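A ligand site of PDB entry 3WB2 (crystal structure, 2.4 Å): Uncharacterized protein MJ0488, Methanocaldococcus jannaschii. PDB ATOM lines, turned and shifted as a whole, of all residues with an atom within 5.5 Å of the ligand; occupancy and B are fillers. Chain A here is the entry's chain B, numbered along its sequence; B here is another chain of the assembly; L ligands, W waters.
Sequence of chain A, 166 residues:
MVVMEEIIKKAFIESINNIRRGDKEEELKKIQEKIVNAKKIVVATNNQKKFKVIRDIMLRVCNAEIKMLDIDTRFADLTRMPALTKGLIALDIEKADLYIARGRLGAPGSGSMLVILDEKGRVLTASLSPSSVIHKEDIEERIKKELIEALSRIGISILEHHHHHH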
ATOM      1  N   LYS A  50       5.578 -10.826  -0.486  1.00  0.00           N
ATOM      2  CA  LYS A  50       4.541  -9.919   0.014  1.00  0.00           C
ATOM      3  C   LYS A  50       3.157 -10.438  -0.423  1.00  0.00           C
ATOM      4  O   LYS A  50       2.258 -10.556   0.410  1.00  0.00           O
ATOM      5  CB  LYS A  50       4.734  -8.464  -0.501  1.00  0.00           C
ATOM      6  CG  LYS A  50       5.852  -7.593   0.137  1.00  0.00           C
ATOM      7  CD  LYS A  50       6.028  -6.281  -0.654  1.00  0.00           C
ATOM      8  CE  LYS A  50       7.029  -5.302  -0.045  1.00  0.00           C
ATOM      9  NZ  LYS A  50       6.924  -3.928  -0.639  1.00  0.00           N
ATOM     10  N   ASP A  77       8.986   4.708  -5.244  1.00  0.00           N
ATOM     11  CA  ASP A  77       9.785   5.050  -4.053  1.00  0.00           C
ATOM     12  C   ASP A  77      10.524   6.417  -4.084  1.00  0.00           C
ATOM     13  O   ASP A  77      11.243   6.709  -3.121  1.00  0.00           O
ATOM     14  CB  ASP A  77      10.773   3.931  -3.653  1.00  0.00           C
ATOM     15  CG  ASP A  77      10.088   2.557  -3.416  1.00  0.00           C
ATOM     16  OD1 ASP A  77       8.844   2.469  -3.154  1.00  0.00           O
ATOM     17  OD2 ASP A  77      10.794   1.531  -3.537  1.00  0.00           O
ATOM     18  N   LYS A  86       2.027   3.536  -4.824  1.00  0.00           N
ATOM     19  CA  LYS A  86       1.927   2.151  -5.284  1.00  0.00           C
ATOM     20  C   LYS A  86       0.460   1.746  -5.492  1.00  0.00           C
ATOM     21  O   LYS A  86       0.087   1.150  -6.507  1.00  0.00           O
ATOM     22  CB  LYS A  86       2.523   1.190  -4.263  1.00  0.00           C
ATOM     23  CG  LYS A  86       4.037   1.213  -4.082  1.00  0.00           C
ATOM     24  CD  LYS A  86       4.374   0.066  -3.149  1.00  0.00           C
ATOM     25  CE  LYS A  86       5.824   0.143  -2.633  1.00  0.00           C
ATOM     26  NZ  LYS A  86       6.719  -0.504  -3.641  1.00  0.00           N
ATOM     27  N   ARG A 102       1.892  -1.935   0.120  1.00  0.00           N
ATOM     28  CA  ARG A 102       2.762  -1.804   1.314  1.00  0.00           C
ATOM     29  C   ARG A 102       4.149  -1.232   0.908  1.00  0.00           C
ATOM     30  O   ARG A 102       4.783  -1.712  -0.049  1.00  0.00           O
ATOM     31  CB  ARG A 102       2.868  -3.150   2.061  1.00  0.00           C
ATOM     32  CG  ARG A 102       3.381  -3.055   3.506  1.00  0.00           C
ATOM     33  CD  ARG A 102       4.932  -3.032   3.610  1.00  0.00           C
ATOM     34  NE  ARG A 102       5.372  -3.243   5.004  1.00  0.00           N
ATOM     35  CZ  ARG A 102       6.655  -3.286   5.442  1.00  0.00           C
ATOM     36  NH1 ARG A 102       6.895  -3.514   6.755  1.00  0.00           N
ATOM     37  NH2 ARG A 102       7.701  -3.121   4.588  1.00  0.00           N
ATOM     38  N   GLY A 103       4.594  -0.192   1.603  1.00  0.00           N
ATOM     39  CA  GLY A 103       5.852   0.502   1.233  1.00  0.00           C
ATOM     40  C   GLY A 103       6.235   1.489   2.307  1.00  0.00           C
ATOM     41  O   GLY A 103       5.720   1.423   3.473  1.00  0.00           O
ATOM     42  N   ARG A 104       7.145   2.397   1.963  1.00  0.00           N
ATOM     43  CA  ARG A 104       7.535   3.493   2.857  1.00  0.00           C
ATOM     44  C   ARG A 104       6.383   4.427   3.112  1.00  0.00           C
ATOM     45  O   ARG A 104       5.583   4.733   2.203  1.00  0.00           O
ATOM     46  CB  ARG A 104       8.713   4.283   2.317  1.00  0.00           C
ATOM     47  CG  ARG A 104       9.381   5.143   3.422  1.00  0.00           C
ATOM     48  CD  ARG A 104      10.748   5.721   3.053  1.00  0.00           C
ATOM     49  NE  ARG A 104      10.686   6.607   1.902  1.00  0.00           N
ATOM     50  CZ  ARG A 104      11.451   6.483   0.798  1.00  0.00           C
ATOM     51  NH1 ARG A 104      12.360   5.491   0.699  1.00  0.00           N
ATOM     52  NH2 ARG A 104      11.317   7.372  -0.230  1.00  0.00           N
ATOM     53  N   PRO A 108      12.567   9.249   3.632  1.00  0.00           N
ATOM     54  CA  PRO A 108      13.459   8.178   4.109  1.00  0.00           C
ATOM     55  C   PRO A 108      13.626   8.164   5.617  1.00  0.00           C
ATOM     56  O   PRO A 108      13.837   9.194   6.209  1.00  0.00           O
ATOM     57  CB  PRO A 108      14.752   8.484   3.410  1.00  0.00           C
ATOM     58  CG  PRO A 108      14.246   8.966   2.081  1.00  0.00           C
ATOM     59  CD  PRO A 108      12.987   9.747   2.323  1.00  0.00           C
ATOM     60  N   GLY A 111       9.667   4.829   8.147  1.00  0.00           N
ATOM     61  CA  GLY A 111       8.971   3.556   8.394  1.00  0.00           C
ATOM     62  C   GLY A 111       8.050   3.147   7.283  1.00  0.00           C
ATOM     63  O   GLY A 111       8.152   3.699   6.176  1.00  0.00           O
ATOM     64  N   SER A 112       7.106   2.244   7.581  1.00  0.00           N
ATOM     65  CA  SER A 112       6.282   1.613   6.571  1.00  0.00           C
ATOM     66  C   SER A 112       4.787   1.891   6.732  1.00  0.00           C
ATOM     67  O   SER A 112       4.313   2.286   7.814  1.00  0.00           O
ATOM     68  CB  SER A 112       6.505   0.122   6.591  1.00  0.00           C
ATOM     69  OG  SER A 112       5.911  -0.426   7.757  1.00  0.00           O
ATOM     70  N   PRO A 130       7.621   1.010  12.566  1.00  0.00           N
ATOM     71  CA  PRO A 130       8.926   1.675  12.586  1.00  0.00           C
ATOM     72  C   PRO A 130       9.909   1.122  11.499  1.00  0.00           C
ATOM     73  O   PRO A 130       9.596   0.125  10.849  1.00  0.00           O
ATOM     74  CB  PRO A 130       9.478   1.379  14.011  1.00  0.00           C
ATOM     75  CG  PRO A 130       8.333   0.809  14.790  1.00  0.00           C
ATOM     76  CD  PRO A 130       7.435   0.149  13.759  1.00  0.00           C
ATOM     77  N   SER A 131      11.039   1.766  11.253  1.00  0.00           N
ATOM     78  CA  SER A 131      12.052   1.189  10.361  1.00  0.00           C
ATOM     79  C   SER A 131      12.493  -0.186  10.887  1.00  0.00           C
ATOM     80  O   SER A 131      12.441  -0.440  12.107  1.00  0.00           O
ATOM     81  CB  SER A 131      13.318   2.080  10.320  1.00  0.00           C
ATOM     82  OG  SER A 131      12.976   3.446  10.267  1.00  0.00           O
ATOM     83  N   SER A 132      12.985  -1.057  10.010  1.00  0.00           N
ATOM     84  CA  SER A 132      13.412  -2.362  10.517  1.00  0.00           C
ATOM     85  C   SER A 132      14.643  -2.282  11.409  1.00  0.00           C
ATOM     86  O   SER A 132      14.804  -3.146  12.258  1.00  0.00           O
ATOM     87  CB  SER A 132      13.598  -3.414   9.391  1.00  0.00           C
ATOM     88  OG  SER A 132      14.577  -2.953   8.457  1.00  0.00           O
ATOM     89  N   HIS A 135      12.688  -2.267  14.731  1.00  0.00           N
ATOM     90  CA  HIS A 135      11.954  -3.462  15.192  1.00  0.00           C
ATOM     91  C   HIS A 135      12.688  -4.790  14.938  1.00  0.00           C
ATOM     92  O   HIS A 135      12.432  -5.795  15.632  1.00  0.00           O
ATOM     93  CB  HIS A 135      10.530  -3.493  14.634  1.00  0.00           C
ATOM     94  CG  HIS A 135      10.435  -3.607  13.139  1.00  0.00           C
ATOM     95  ND1 HIS A 135      10.820  -4.728  12.448  1.00  0.00           N
ATOM     96  CD2 HIS A 135       9.953  -2.760  12.212  1.00  0.00           C
ATOM     97  CE1 HIS A 135      10.601  -4.569  11.167  1.00  0.00           C
ATOM     98  NE2 HIS A 135      10.058  -3.375  10.991  1.00  0.00           N
ATOM     99  N   GLU A 137      12.405  -7.222  12.902  1.00  0.00           N
ATOM    100  CA  GLU A 137      11.696  -8.433  12.495  1.00  0.00           C
ATOM    101  C   GLU A 137      11.818  -8.652  11.003  1.00  0.00           C
ATOM    102  O   GLU A 137      12.049  -7.690  10.261  1.00  0.00           O
ATOM    103  CB  GLU A 137      10.223  -8.323  12.862  1.00  0.00           C
ATOM    104  CG  GLU A 137       9.935  -8.420  14.348  1.00  0.00           C
ATOM    105  CD  GLU A 137       8.489  -8.116  14.700  1.00  0.00           C
ATOM    106  OE1 GLU A 137       7.558  -8.686  14.106  1.00  0.00           O
ATOM    107  OE2 GLU A 137       8.245  -7.310  15.592  1.00  0.00           O
ATOM    108  N   ASP A 138      11.612  -9.891  10.548  1.00  0.00           N
ATOM    109  CA  ASP A 138      11.494 -10.216   9.082  1.00  0.00           C
ATOM    110  C   ASP A 138      10.327  -9.485   8.476  1.00  0.00           C
ATOM    111  O   ASP A 138       9.343  -9.206   9.169  1.00  0.00           O
ATOM    112  CB  ASP A 138      11.202 -11.713   8.809  1.00  0.00           C
ATOM    113  CG  ASP A 138      12.392 -12.621   9.019  1.00  0.00           C
ATOM    114  OD1 ASP A 138      13.448 -12.224   9.583  1.00  0.00           O
ATOM    115  OD2 ASP A 138      12.218 -13.809   8.641  1.00  0.00           O
ATOM    116  N   ILE A 139      10.423  -9.238   7.175  1.00  0.00           N
ATOM    117  CA  ILE A 139       9.388  -8.484   6.476  1.00  0.00           C
ATOM    118  C   ILE A 139       8.070  -9.274   6.420  1.00  0.00           C
ATOM    119  O   ILE A 139       7.013  -8.678   6.596  1.00  0.00           O
ATOM    120  CB  ILE A 139       9.850  -7.932   5.108  1.00  0.00           C
ATOM    121  CG1 ILE A 139       8.927  -6.816   4.631  1.00  0.00           C
ATOM    122  CG2 ILE A 139       9.978  -9.053   4.042  1.00  0.00           C
ATOM    123  CD1 ILE A 139       9.355  -6.101   3.340  1.00  0.00           C
ATOM    124  N   ARG A 142       6.194  -8.686   9.827  1.00  0.00           N
ATOM    125  CA  ARG A 142       5.689  -7.362   9.934  1.00  0.00           C
ATOM    126  C   ARG A 142       4.470  -7.115   9.053  1.00  0.00           C
ATOM    127  O   ARG A 142       3.494  -6.515   9.524  1.00  0.00           O
ATOM    128  CB  ARG A 142       6.803  -6.418   9.521  1.00  0.00           C
ATOM    129  CG  ARG A 142       6.866  -5.137  10.300  1.00  0.00           C
ATOM    130  CD  ARG A 142       7.209  -5.382  11.784  1.00  0.00           C
ATOM    131  NE  ARG A 142       6.330  -4.487  12.496  1.00  0.00           N
ATOM    132  CZ  ARG A 142       6.273  -4.294  13.806  1.00  0.00           C
ATOM    133  NH1 ARG A 142       7.051  -4.966  14.647  1.00  0.00           N
ATOM    134  NH2 ARG A 142       5.418  -3.416  14.269  1.00  0.00           N
ATOM    135  N   SER B  15      17.539   3.450  -4.405  1.00  0.00           N
ATOM    136  CA  SER B  15      16.386   2.980  -5.211  1.00  0.00           C
ATOM    137  C   SER B  15      16.666   2.918  -6.718  1.00  0.00           C
ATOM    138  O   SER B  15      16.349   1.945  -7.366  1.00  0.00           O
ATOM    139  CB  SER B  15      15.156   3.836  -5.006  1.00  0.00           C
ATOM    140  OG  SER B  15      14.799   3.884  -3.650  1.00  0.00           O
ATOM    141  N   ARG B  20      17.962  -0.518  -2.552  1.00  0.00           N
ATOM    142  CA  ARG B  20      17.331   0.029  -1.339  1.00  0.00           C
ATOM    143  C   ARG B  20      16.693  -1.057  -0.409  1.00  0.00           C
ATOM    144  O   ARG B  20      15.506  -1.420  -0.550  1.00  0.00           O
ATOM    145  CB  ARG B  20      16.310   1.106  -1.718  1.00  0.00           C
ATOM    146  CG  ARG B  20      15.702   1.863  -0.535  1.00  0.00           C
ATOM    147  CD  ARG B  20      16.627   2.690   0.328  1.00  0.00           C
ATOM    148  NE  ARG B  20      15.838   3.337   1.390  1.00  0.00           N
ATOM    149  CZ  ARG B  20      16.305   4.202   2.276  1.00  0.00           C
ATOM    150  NH1 ARG B  20      17.557   4.549   2.217  1.00  0.00           N
ATOM    151  NH2 ARG B  20      15.515   4.746   3.188  1.00  0.00           N
ATOM    152  N   ARG B  21      17.509  -1.546   0.548  1.00  0.00           N
ATOM    153  CA  ARG B  21      17.087  -2.610   1.461  1.00  0.00           C
ATOM    154  C   ARG B  21      16.722  -2.083   2.865  1.00  0.00           C
ATOM    155  O   ARG B  21      17.059  -2.727   3.873  1.00  0.00           O
ATOM    156  CB  ARG B  21      18.160  -3.707   1.534  1.00  0.00           C
ATOM    157  CG  ARG B  21      18.593  -4.258   0.189  1.00  0.00           C
ATOM    158  CD  ARG B  21      17.759  -5.456  -0.278  1.00  0.00           C
ATOM    159  NE  ARG B  21      16.337  -5.155  -0.558  1.00  0.00           N
ATOM    160  CZ  ARG B  21      15.843  -4.747  -1.743  1.00  0.00           C
ATOM    161  NH1 ARG B  21      16.656  -4.524  -2.776  1.00  0.00           N
ATOM    162  NH2 ARG B  21      14.537  -4.537  -1.882  1.00  0.00           N
ATOM    163  N   GLY B  22      16.006  -0.946   2.921  1.00  0.00           N
ATOM    164  CA  GLY B  22      15.409  -0.417   4.173  1.00  0.00           C
ATOM    165  C   GLY B  22      15.976   0.937   4.581  1.00  0.00           C
ATOM    166  O   GLY B  22      16.997   1.381   4.031  1.00  0.00           O
ATOM    167  N   ASP B  23      15.310   1.590   5.541  1.00  0.00           N
ATOM    168  CA  ASP B  23      15.743   2.840   6.112  1.00  0.00           C
ATOM    169  C   ASP B  23      17.119   2.708   6.793  1.00  0.00           C
ATOM    170  O   ASP B  23      17.416   1.669   7.369  1.00  0.00           O
ATOM    171  CB  ASP B  23      14.740   3.341   7.180  1.00  0.00           C
ATOM    172  CG  ASP B  23      13.345   3.650   6.608  1.00  0.00           C
ATOM    173  OD1 ASP B  23      13.197   3.895   5.379  1.00  0.00           O
ATOM    174  OD2 ASP B  23      12.406   3.636   7.450  1.00  0.00           O
HETATM  175  C1  LIG L   1      13.037  -6.163   7.111  1.00  0.00           C
HETATM  176  N1  LIG L   1      13.918  -7.070   7.529  1.00  0.00           N
HETATM  177  C2  LIG L   1      12.351  -4.488   5.622  1.00  0.00           C
HETATM  178  C3  LIG L   1      11.157  -4.316   6.251  1.00  0.00           C
HETATM  179  C4  LIG L   1      10.886  -5.062   7.340  1.00  0.00           C
HETATM  180  O1  LIG L   1       9.832  -4.919   7.940  1.00  0.00           O
HETATM  181  N2  LIG L   1      11.809  -6.039   7.803  1.00  0.00           N
HETATM  182  N3  LIG L   1      13.255  -5.381   6.026  1.00  0.00           N
HETATM  183  N4  LIG L   1      10.456  -3.348   5.638  1.00  0.00           N
HETATM  184  C5  LIG L   1      11.201  -2.960   4.613  1.00  0.00           C
HETATM  185  N5  LIG L   1      12.360  -3.655   4.596  1.00  0.00           N
HETATM  186  C6  LIG L   1      13.501  -3.559   3.618  1.00  0.00           C
HETATM  187  O2  LIG L   1      13.386  -2.399   2.698  1.00  0.00           O
HETATM  188  C7  LIG L   1      13.478  -4.814   2.742  1.00  0.00           C
HETATM  189  O3  LIG L   1      14.768  -5.120   2.333  1.00  0.00           O
HETATM  190  C8  LIG L   1      12.639  -4.362   1.580  1.00  0.00           C
HETATM  191  O4  LIG L   1      12.881  -5.162   0.403  1.00  0.00           O
HETATM  192  C9  LIG L   1      13.125  -2.919   1.355  1.00  0.00           C
HETATM  193  C10 LIG L   1      11.978  -2.135   0.768  1.00  0.00           C
HETATM  194  O5  LIG L   1      10.751  -2.415   1.509  1.00  0.00           O
HETATM  195  P1  LIG L   1       9.405  -1.684   1.004  1.00  0.00           P
HETATM  196  O6  LIG L   1       8.279  -1.897   2.043  1.00  0.00           O
HETATM  197  O7  LIG L   1       8.966  -2.136  -0.314  1.00  0.00           O
HETATM  198  O8  LIG L   1       9.762  -0.077   1.000  1.00  0.00           O
HETATM  199  C11 LIG L   1      10.405   0.650   1.970  1.00  0.00           C
HETATM  200  C12 LIG L   1      10.106   0.572   3.340  1.00  0.00           C
HETATM  201  C13 LIG L   1      10.820   1.357   4.267  1.00  0.00           C
HETATM  202  C14 LIG L   1      10.564   1.286   5.644  1.00  0.00           C
HETATM  203  N6  LIG L   1      11.802   2.265   3.768  1.00  0.00           N
HETATM  204  C15 LIG L   1      12.096   2.355   2.393  1.00  0.00           C
HETATM  205  O9  LIG L   1      12.960   3.168   2.038  1.00  0.00           O
HETATM  206  C16 LIG L   1      11.379   1.536   1.469  1.00  0.00           C
HETATM  207  C17 LIG L   1      11.595   1.560   0.051  1.00  0.00           C
HETATM  208  O   HOH W   1       9.585  -0.697  -2.713  1.00  0.00           O
HETATM  209  O   HOH W   2       8.297   1.917  -0.851  1.00  0.00           O
HETATM  210  O   HOH W   3      15.904  -7.967   5.025  1.00  0.00           O
HETATM  211  O   HOH W   4      13.017  -9.885   6.129  1.00  0.00           O
HETATM  212  O   HOH W   5       9.532  -1.723   8.639  1.00  0.00           O
HETATM  213  O   HOH W   6      17.120  -6.606   8.597  1.00  0.00           O
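Residues that only touch the ligand: Asp 77 (3.7 Å), Gly 103 (3.5 Å), Gly 111 (3.5 Å), Ser 132 (3.6 Å), Asp 138 (3.8 Å), Ile 139 (3.5 Å) and Arg 142 (3.7 Å).
Hydrophobic or aromatic side chains that line the ligand: His 135 and Ile 139.
Along chain A the residues within 4 Å of the ligand span positions 50 to 142.
NZ of Lys 86 is in salt-bridge range of OD1 of Asp 77, 3.7 Å away.
The side-chain amino group (NZ) of Lys 50 sits at hydrogen-bond distance from the backbone carbonyl oxygen (O) of Arg 102 (3.1 Å).
OE2 of Glu 137 is in salt-bridge range of NH1 of Arg 142 (2.8 Å).
The guanidinium group (NE) of Arg 20 of chain B lies close to the backbone carbonyl oxygen (O) of Gly 22 of chain B (3.5 Å).
OD2 of Asp 23 of chain B sits at hydrogen-bond distance from OG of Ser 131, 2.9 Å away.
A ring nitrogen (ND1) of His 135 is in hydrogen-bond range of the backbone NH (N) of Glu 137 (3.0 Å).
The guanidinium group of Arg 20 of chain B is in salt-bridge range of the side-chain carboxylate of Asp 23 of chain B (3.3 Å).
The side-chain hydroxyl (OG) of Ser 112 lies within hydrogen-bond range of the guanidinium group (NH1) of Arg 102, 3.4 Å away.
O4 of the ligand lies within hydrogen-bond range of NH2 of Arg 21 of chain B.
An oxygen (O9) of the ligand lies within hydrogen-bond range of the guanidinium group (NH1) of Arg 104 (2.7 Å).
A nitrogen (N2) of the ligand lies within hydrogen-bond range of the backbone carbonyl oxygen (O) of Glu 137.
The side-chain carboxylate of Asp 23 of chain B sits at hydrogen-bond distance from a nitrogen (N6) of the ligand (2.7 Å).
A ring nitrogen (NE2) of His 135 lies close to an oxygen (O1) of the ligand, at 3.4 Å.
The side-chain amino group (NZ) of Lys 50 is in salt-bridge range of an oxygen (O7) of the ligand (2.7 Å).
An oxygen (O2) of the ligand sits at hydrogen-bond distance from the backbone NH (N) of Gly 22 of chain B (3.0 Å).
An oxygen (O6) of the ligand is in salt-bridge range of the guanidinium group (NH2) of Arg 102 (2.9 Å).
The guanidinium group of Arg 20 of chain B is in hydrogen-bond range of an oxygen (O9) of the ligand, 3.0 Å away.
Water W1 lies within hydrogen-bond range of OD2 of Asp 77 (2.7 Å), O7 of the ligand (2.9 Å) and NZ of Lys 86 (3.0 Å).
Water W2 lies within hydrogen-bond range of OD1 of Asp 77, N of Arg 104 and O8 of the ligand.
Water W4 bridges the backbone NH (N) of Ile 139 and a nitrogen (N1) of the ligand.
Water W5 lies within hydrogen-bond range of the backbone carbonyl oxygen of Pro 130 (2.9 Å), a ring nitrogen (NE2) of His 135 (2.9 Å) and an oxygen (O1) of the ligand (3.3 Å).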
